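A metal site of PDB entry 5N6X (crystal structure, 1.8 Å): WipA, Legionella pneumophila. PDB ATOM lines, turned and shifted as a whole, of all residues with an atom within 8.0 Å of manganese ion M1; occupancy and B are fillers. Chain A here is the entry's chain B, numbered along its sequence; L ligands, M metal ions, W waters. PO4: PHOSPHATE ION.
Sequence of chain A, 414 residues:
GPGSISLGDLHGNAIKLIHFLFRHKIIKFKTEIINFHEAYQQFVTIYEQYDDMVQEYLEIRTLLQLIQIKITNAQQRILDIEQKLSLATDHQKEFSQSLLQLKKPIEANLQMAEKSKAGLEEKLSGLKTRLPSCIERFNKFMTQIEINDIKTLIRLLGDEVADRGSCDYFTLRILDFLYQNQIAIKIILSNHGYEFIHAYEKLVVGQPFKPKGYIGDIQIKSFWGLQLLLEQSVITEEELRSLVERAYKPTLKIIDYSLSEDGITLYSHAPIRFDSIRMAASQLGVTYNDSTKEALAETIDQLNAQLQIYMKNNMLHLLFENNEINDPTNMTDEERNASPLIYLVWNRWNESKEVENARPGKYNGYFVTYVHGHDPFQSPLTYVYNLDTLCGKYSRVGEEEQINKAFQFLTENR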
ATOM      1  N   GLY A   8     -16.926  -5.367  19.701  1.00  0.00           N
ATOM      2  CA  GLY A   8     -15.631  -5.142  20.323  1.00  0.00           C
ATOM      3  C   GLY A   8     -14.478  -5.905  19.733  1.00  0.00           C
ATOM      4  O   GLY A   8     -13.367  -5.856  20.265  1.00  0.00           O
ATOM      5  N   HIS A  11     -11.000  -5.707  14.262  1.00  0.00           N
ATOM      6  CA  HIS A  11      -9.631  -5.804  13.765  1.00  0.00           C
ATOM      7  C   HIS A  11      -9.561  -5.651  12.241  1.00  0.00           C
ATOM      8  O   HIS A  11      -8.930  -6.435  11.526  1.00  0.00           O
ATOM      9  CB  HIS A  11      -8.966  -7.101  14.238  1.00  0.00           C
ATOM     10  CG  HIS A  11      -9.124  -7.407  15.714  1.00  0.00           C
ATOM     11  ND1 HIS A  11      -8.372  -6.832  16.736  1.00  0.00           N
ATOM     12  CD2 HIS A  11      -9.938  -8.300  16.331  1.00  0.00           C
ATOM     13  CE1 HIS A  11      -8.741  -7.344  17.912  1.00  0.00           C
ATOM     14  NE2 HIS A  11      -9.704  -8.223  17.678  1.00  0.00           N
ATOM     15  N   LEU A 157     -16.537  -0.513  18.895  1.00  0.00           N
ATOM     16  CA  LEU A 157     -15.670  -0.111  20.001  1.00  0.00           C
ATOM     17  C   LEU A 157     -14.237   0.150  19.554  1.00  0.00           C
ATOM     18  O   LEU A 157     -13.407   0.529  20.392  1.00  0.00           O
ATOM     19  CB  LEU A 157     -15.699  -1.152  21.133  1.00  0.00           C
ATOM     20  CG  LEU A 157     -17.109  -1.329  21.694  1.00  0.00           C
ATOM     21  CD1 LEU A 157     -17.110  -2.387  22.823  1.00  0.00           C
ATOM     22  CD2 LEU A 157     -17.713  -0.017  22.197  1.00  0.00           C
ATOM     23  N   GLY A 158     -13.926  -0.026  18.274  1.00  0.00           N
ATOM     24  CA  GLY A 158     -12.658   0.457  17.768  1.00  0.00           C
ATOM     25  C   GLY A 158     -11.872  -0.599  17.026  1.00  0.00           C
ATOM     26  O   GLY A 158     -12.308  -1.741  16.840  1.00  0.00           O
ATOM     27  N   ASP A 159     -10.675  -0.190  16.581  1.00  0.00           N
ATOM     28  CA  ASP A 159      -9.812  -0.983  15.698  1.00  0.00           C
ATOM     29  C   ASP A 159     -10.574  -1.482  14.475  1.00  0.00           C
ATOM     30  O   ASP A 159     -10.355  -2.604  13.978  1.00  0.00           O
ATOM     31  CB  ASP A 159      -9.122  -2.117  16.475  1.00  0.00           C
ATOM     32  CG  ASP A 159      -8.122  -1.606  17.558  1.00  0.00           C
ATOM     33  OD1 ASP A 159      -7.705  -0.442  17.638  1.00  0.00           O
ATOM     34  OD2 ASP A 159      -7.671  -2.383  18.381  1.00  0.00           O
ATOM     35  N   GLU A 160     -11.455  -0.616  13.936  1.00  0.00           N
ATOM     36  CA  GLU A 160     -12.277  -0.895  12.766  1.00  0.00           C
ATOM     37  C   GLU A 160     -11.512  -0.737  11.451  1.00  0.00           C
ATOM     38  O   GLU A 160     -11.970  -1.253  10.425  1.00  0.00           O
ATOM     39  CB  GLU A 160     -13.492   0.056  12.749  1.00  0.00           C
ATOM     40  CG  GLU A 160     -13.155   1.542  12.529  1.00  0.00           C
ATOM     41  CD  GLU A 160     -12.551   2.222  13.757  1.00  0.00           C
ATOM     42  OE1 GLU A 160     -12.605   1.665  14.877  1.00  0.00           O
ATOM     43  OE2 GLU A 160     -12.020   3.352  13.621  1.00  0.00           O
ATOM     44  N   ASP A 163      -5.936  -2.298  10.665  1.00  0.00           N
ATOM     45  CA  ASP A 163      -5.709  -3.437  11.564  1.00  0.00           C
ATOM     46  C   ASP A 163      -5.413  -4.634  10.675  1.00  0.00           C
ATOM     47  O   ASP A 163      -4.934  -4.493   9.554  1.00  0.00           O
ATOM     48  CB  ASP A 163      -6.902  -3.573  12.540  1.00  0.00           C
ATOM     49  CG  ASP A 163      -6.564  -4.377  13.813  1.00  0.00           C
ATOM     50  OD1 ASP A 163      -6.034  -5.490  13.715  1.00  0.00           O
ATOM     51  OD2 ASP A 163      -6.888  -3.907  14.933  1.00  0.00           O
ATOM     52  N   ARG A 164      -5.670  -5.840  11.176  1.00  0.00           N
ATOM     53  CA  ARG A 164      -5.034  -7.029  10.590  1.00  0.00           C
ATOM     54  C   ARG A 164      -5.788  -7.618   9.400  1.00  0.00           C
ATOM     55  O   ARG A 164      -5.228  -8.508   8.735  1.00  0.00           O
ATOM     56  CB  ARG A 164      -4.826  -8.100  11.677  1.00  0.00           C
ATOM     57  CG  ARG A 164      -3.828  -7.646  12.750  1.00  0.00           C
ATOM     58  CD  ARG A 164      -4.108  -8.274  14.116  1.00  0.00           C
ATOM     59  NE  ARG A 164      -3.128  -7.858  15.137  1.00  0.00           N
ATOM     60  CZ  ARG A 164      -3.308  -6.858  15.995  1.00  0.00           C
ATOM     61  NH1 ARG A 164      -4.433  -6.155  15.993  1.00  0.00           N
ATOM     62  NH2 ARG A 164      -2.351  -6.576  16.886  1.00  0.00           N
ATOM     63  N   LEU A 189     -12.826   6.112  19.159  1.00  0.00           N
ATOM     64  CA  LEU A 189     -11.440   6.327  18.746  1.00  0.00           C
ATOM     65  C   LEU A 189     -10.552   5.255  19.380  1.00  0.00           C
ATOM     66  O   LEU A 189     -10.696   4.903  20.562  1.00  0.00           O
ATOM     67  CB  LEU A 189     -11.006   7.742  19.178  1.00  0.00           C
ATOM     68  CG  LEU A 189      -9.657   8.331  18.773  1.00  0.00           C
ATOM     69  CD1 LEU A 189      -9.515   8.298  17.261  1.00  0.00           C
ATOM     70  CD2 LEU A 189      -9.527   9.761  19.304  1.00  0.00           C
ATOM     71  N   SER A 190      -9.609   4.736  18.586  1.00  0.00           N
ATOM     72  CA  SER A 190      -8.835   3.563  18.989  1.00  0.00           C
ATOM     73  C   SER A 190      -7.396   3.705  18.518  1.00  0.00           C
ATOM     74  O   SER A 190      -7.054   4.644  17.789  1.00  0.00           O
ATOM     75  CB  SER A 190      -9.451   2.289  18.405  1.00  0.00           C
ATOM     76  OG  SER A 190      -9.496   2.395  16.973  1.00  0.00           O
ATOM     77  N   ASN A 191      -6.530   2.758  18.931  1.00  0.00           N
ATOM     78  CA  ASN A 191      -5.127   2.913  18.556  1.00  0.00           C
ATOM     79  C   ASN A 191      -4.927   2.584  17.075  1.00  0.00           C
ATOM     80  O   ASN A 191      -4.124   3.242  16.413  1.00  0.00           O
ATOM     81  CB  ASN A 191      -4.195   2.076  19.457  1.00  0.00           C
ATOM     82  CG  ASN A 191      -4.553   0.590  19.490  1.00  0.00           C
ATOM     83  OD1 ASN A 191      -5.735   0.220  19.472  1.00  0.00           O
ATOM     84  ND2 ASN A 191      -3.524  -0.262  19.566  1.00  0.00           N
ATOM     85  N   HIS A 192      -5.658   1.605  16.537  1.00  0.00           N
ATOM     86  CA  HIS A 192      -5.571   1.380  15.097  1.00  0.00           C
ATOM     87  C   HIS A 192      -6.350   2.444  14.333  1.00  0.00           C
ATOM     88  O   HIS A 192      -5.905   2.898  13.256  1.00  0.00           O
ATOM     89  CB  HIS A 192      -6.074  -0.027  14.734  1.00  0.00           C
ATOM     90  CG  HIS A 192      -5.160  -1.113  15.202  1.00  0.00           C
ATOM     91  ND1 HIS A 192      -4.339  -1.822  14.342  1.00  0.00           N
ATOM     92  CD2 HIS A 192      -4.908  -1.596  16.442  1.00  0.00           C
ATOM     93  CE1 HIS A 192      -3.633  -2.698  15.031  1.00  0.00           C
ATOM     94  NE2 HIS A 192      -3.960  -2.587  16.307  1.00  0.00           N
ATOM     95  N   GLY A 193      -7.504   2.857  14.859  1.00  0.00           N
ATOM     96  CA  GLY A 193      -8.194   3.988  14.261  1.00  0.00           C
ATOM     97  C   GLY A 193      -7.282   5.188  14.099  1.00  0.00           C
ATOM     98  O   GLY A 193      -7.273   5.839  13.048  1.00  0.00           O
ATOM     99  N   ILE A 215       2.451   1.290  14.996  1.00  0.00           N
ATOM    100  CA  ILE A 215       2.042  -0.086  14.819  1.00  0.00           C
ATOM    101  C   ILE A 215       2.693  -0.641  13.559  1.00  0.00           C
ATOM    102  O   ILE A 215       2.772   0.049  12.534  1.00  0.00           O
ATOM    103  CB  ILE A 215       0.504  -0.192  14.743  1.00  0.00           C
ATOM    104  CG1 ILE A 215      -0.136   0.441  15.989  1.00  0.00           C
ATOM    105  CG2 ILE A 215       0.091  -1.624  14.590  1.00  0.00           C
ATOM    106  CD1 ILE A 215      -1.670   0.398  15.981  1.00  0.00           C
ATOM    107  N   HIS A 269     -12.602   2.175  24.094  1.00  0.00           N
ATOM    108  CA  HIS A 269     -11.900   1.181  23.275  1.00  0.00           C
ATOM    109  C   HIS A 269     -11.047   0.278  24.161  1.00  0.00           C
ATOM    110  O   HIS A 269     -11.263  -0.939  24.219  1.00  0.00           O
ATOM    111  CB  HIS A 269     -11.010   1.833  22.213  1.00  0.00           C
ATOM    112  CG  HIS A 269     -10.172   0.837  21.474  1.00  0.00           C
ATOM    113  ND1 HIS A 269     -10.735  -0.194  20.753  1.00  0.00           N
ATOM    114  CD2 HIS A 269      -8.828   0.631  21.430  1.00  0.00           C
ATOM    115  CE1 HIS A 269      -9.770  -0.948  20.235  1.00  0.00           C
ATOM    116  NE2 HIS A 269      -8.606  -0.463  20.636  1.00  0.00           N
ATOM    117  N   ALA A 270     -10.062   0.862  24.824  1.00  0.00           N
ATOM    118  CA  ALA A 270      -9.275   0.181  25.831  1.00  0.00           C
ATOM    119  C   ALA A 270     -10.064   0.089  27.131  1.00  0.00           C
ATOM    120  O   ALA A 270     -10.943   0.909  27.398  1.00  0.00           O
ATOM    121  CB  ALA A 270      -7.969   0.938  26.077  1.00  0.00           C
ATOM    122  N   PRO A 271      -9.751  -0.886  27.991  1.00  0.00           N
ATOM    123  CA  PRO A 271     -10.249  -0.794  29.370  1.00  0.00           C
ATOM    124  C   PRO A 271      -9.608   0.413  30.068  1.00  0.00           C
ATOM    125  O   PRO A 271      -8.389   0.603  29.984  1.00  0.00           O
ATOM    126  CB  PRO A 271      -9.803  -2.124  30.008  1.00  0.00           C
ATOM    127  CG  PRO A 271      -8.537  -2.479  29.239  1.00  0.00           C
ATOM    128  CD  PRO A 271      -8.817  -2.017  27.801  1.00  0.00           C
ATOM    129  N   LEU A 344      -6.329   6.234  26.659  1.00  0.00           N
ATOM    130  CA  LEU A 344      -7.656   5.725  26.340  1.00  0.00           C
ATOM    131  C   LEU A 344      -7.674   4.727  25.195  1.00  0.00           C
ATOM    132  O   LEU A 344      -8.610   3.928  25.105  1.00  0.00           O
ATOM    133  CB  LEU A 344      -8.598   6.860  25.984  1.00  0.00           C
ATOM    134  CG  LEU A 344      -8.974   7.846  27.082  1.00  0.00           C
ATOM    135  CD1 LEU A 344      -9.947   8.845  26.508  1.00  0.00           C
ATOM    136  CD2 LEU A 344      -9.582   7.151  28.253  1.00  0.00           C
ATOM    137  N   VAL A 345      -6.690   4.758  24.288  1.00  0.00           N
ATOM    138  CA  VAL A 345      -6.718   3.859  23.139  1.00  0.00           C
ATOM    139  C   VAL A 345      -5.699   2.737  23.222  1.00  0.00           C
ATOM    140  O   VAL A 345      -5.783   1.801  22.418  1.00  0.00           O
ATOM    141  CB  VAL A 345      -6.570   4.602  21.794  1.00  0.00           C
ATOM    142  CG1 VAL A 345      -7.594   5.719  21.670  1.00  0.00           C
ATOM    143  CG2 VAL A 345      -5.138   5.145  21.587  1.00  0.00           C
ATOM    144  N   TRP A 346      -4.754   2.792  24.177  1.00  0.00           N
ATOM    145  CA  TRP A 346      -3.687   1.800  24.254  1.00  0.00           C
ATOM    146  C   TRP A 346      -3.696   0.921  25.487  1.00  0.00           C
ATOM    147  O   TRP A 346      -3.093  -0.172  25.457  1.00  0.00           O
ATOM    148  CB  TRP A 346      -2.316   2.504  24.171  1.00  0.00           C
ATOM    149  CG  TRP A 346      -1.904   2.741  22.769  1.00  0.00           C
ATOM    150  CD1 TRP A 346      -2.023   3.910  22.056  1.00  0.00           C
ATOM    151  CD2 TRP A 346      -1.301   1.794  21.883  1.00  0.00           C
ATOM    152  NE1 TRP A 346      -1.543   3.736  20.783  1.00  0.00           N
ATOM    153  CE2 TRP A 346      -1.087   2.453  20.650  1.00  0.00           C
ATOM    154  CE3 TRP A 346      -0.925   0.440  22.013  1.00  0.00           C
ATOM    155  CZ2 TRP A 346      -0.515   1.803  19.555  1.00  0.00           C
ATOM    156  CZ3 TRP A 346      -0.346  -0.198  20.918  1.00  0.00           C
ATOM    157  CH2 TRP A 346      -0.153   0.490  19.705  1.00  0.00           C
ATOM    158  N   ASN A 347      -4.352   1.341  26.565  1.00  0.00           N
ATOM    159  CA  ASN A 347      -4.224   0.642  27.837  1.00  0.00           C
ATOM    160  C   ASN A 347      -4.619  -0.827  27.705  1.00  0.00           C
ATOM    161  O   ASN A 347      -5.585  -1.164  27.006  1.00  0.00           O
ATOM    162  CB  ASN A 347      -5.112   1.290  28.891  1.00  0.00           C
ATOM    163  CG  ASN A 347      -4.728   0.897  30.299  1.00  0.00           C
ATOM    164  OD1 ASN A 347      -3.541   0.835  30.627  1.00  0.00           O
ATOM    165  ND2 ASN A 347      -5.729   0.644  31.143  1.00  0.00           N
ATOM    166  N   ARG A 348      -3.869  -1.697  28.374  1.00  0.00           N
ATOM    167  CA  ARG A 348      -4.218  -3.106  28.509  1.00  0.00           C
ATOM    168  C   ARG A 348      -4.292  -3.431  30.003  1.00  0.00           C
ATOM    169  O   ARG A 348      -3.365  -3.103  30.750  1.00  0.00           O
ATOM    170  CB  ARG A 348      -3.189  -4.022  27.816  1.00  0.00           C
ATOM    171  CG  ARG A 348      -3.131  -3.821  26.290  1.00  0.00           C
ATOM    172  CD  ARG A 348      -2.345  -4.944  25.626  1.00  0.00           C
ATOM    173  NE  ARG A 348      -1.934  -4.606  24.273  1.00  0.00           N
ATOM    174  CZ  ARG A 348      -0.856  -5.129  23.675  1.00  0.00           C
ATOM    175  NH1 ARG A 348      -0.551  -4.760  22.435  1.00  0.00           N
ATOM    176  NH2 ARG A 348      -0.090  -6.000  24.311  1.00  0.00           N
ATOM    177  N   GLY A 373     -13.677  -2.600  24.238  1.00  0.00           N
ATOM    178  CA  GLY A 373     -13.259  -3.580  23.252  1.00  0.00           C
ATOM    179  C   GLY A 373     -12.429  -4.691  23.877  1.00  0.00           C
ATOM    180  O   GLY A 373     -11.867  -4.540  24.963  1.00  0.00           O
ATOM    181  N   HIS A 374     -12.350  -5.806  23.172  1.00  0.00           N
ATOM    182  CA  HIS A 374     -11.737  -7.014  23.726  1.00  0.00           C
ATOM    183  C   HIS A 374     -10.336  -6.713  24.278  1.00  0.00           C
ATOM    184  O   HIS A 374      -9.556  -5.957  23.692  1.00  0.00           O
ATOM    185  CB  HIS A 374     -11.713  -8.089  22.633  1.00  0.00           C
ATOM    186  CG  HIS A 374     -10.664  -9.147  22.838  1.00  0.00           C
ATOM    187  ND1 HIS A 374      -9.584  -9.284  22.002  1.00  0.00           N
ATOM    188  CD2 HIS A 374     -10.549 -10.116  23.782  1.00  0.00           C
ATOM    189  CE1 HIS A 374      -8.835 -10.284  22.432  1.00  0.00           C
ATOM    190  NE2 HIS A 374      -9.402 -10.803  23.507  1.00  0.00           N
ATOM    191  N   ASP A 375     -10.053  -7.289  25.447  1.00  0.00           N
ATOM    192  CA  ASP A 375      -8.767  -7.168  26.130  1.00  0.00           C
ATOM    193  C   ASP A 375      -8.500  -8.520  26.784  1.00  0.00           C
ATOM    194  O   ASP A 375      -9.436  -9.119  27.342  1.00  0.00           O
ATOM    195  CB  ASP A 375      -8.793  -6.041  27.175  1.00  0.00           C
ATOM    196  CG  ASP A 375      -7.418  -5.766  27.789  1.00  0.00           C
ATOM    197  OD1 ASP A 375      -6.427  -5.632  27.036  1.00  0.00           O
ATOM    198  OD2 ASP A 375      -7.345  -5.654  29.031  1.00  0.00           O
HETATM  199  P   PO4 L   1      -4.670  -4.102  19.211  1.00  0.00           P
HETATM  200  O1  PO4 L   1      -4.956  -2.765  19.835  1.00  0.00           O
HETATM  201  O2  PO4 L   1      -4.583  -5.139  20.311  1.00  0.00           O
HETATM  202  O3  PO4 L   1      -5.773  -4.491  18.226  1.00  0.00           O
HETATM  203  O4  PO4 L   1      -3.350  -4.090  18.451  1.00  0.00           O
HETATM  204 MN    MN M   1      -6.762  -1.592  20.225  1.00  0.00          MN
HETATM  205 MN    MN M   2      -9.349  -8.457  19.728  1.00  0.00          MN
HETATM  206  O   HOH W   1      -5.823  -0.914  22.190  1.00  0.00           O
HETATM  207  O   HOH W   2      -7.678  -3.214  21.478  1.00  0.00           O
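Manganese ion M1 is bound by an oxygen (O1) of the ligand (2.2 Å), a ring nitrogen (NE2) of His 269 (2.2 Å), the side-chain carboxylate (OD2) of Asp 159 (2.2 Å), the side-chain amide oxygen (OD1) of Asn 191 (2.2 Å), water W2 (2.2 Å) and water W1 (2.3 Å).
Within 4 Å of manganese ion M1: Asp 159, Asn 191 and His 269. The nearest printed residue that does not touch manganese ion M1 is Val 345 (4.2 Å).
The backbone carbonyl oxygen (O) of Leu 157 is in hydrogen-bond range of a ring nitrogen (ND1) of His 269 (2.8 Å). The backbone NH of Gly 373 lies within hydrogen-bond range of the backbone carbonyl oxygen of His 269, 2.9 Å away. The side-chain carboxylate (OD1) of Asp 159 lies within hydrogen-bond range of the backbone NH (N) of His 192 (3.1 Å). OG of Ser 190 is in hydrogen-bond range of N of Asp 159 (2.9 Å). The backbone carbonyl oxygen (O) of Asp 159 sits at hydrogen-bond distance from the backbone NH (N) of His 11, 3.2 Å away. The side-chain amide oxygen of Asn 191 sits close to the backbone carbonyl oxygen of Val 345 (3.3 Å).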
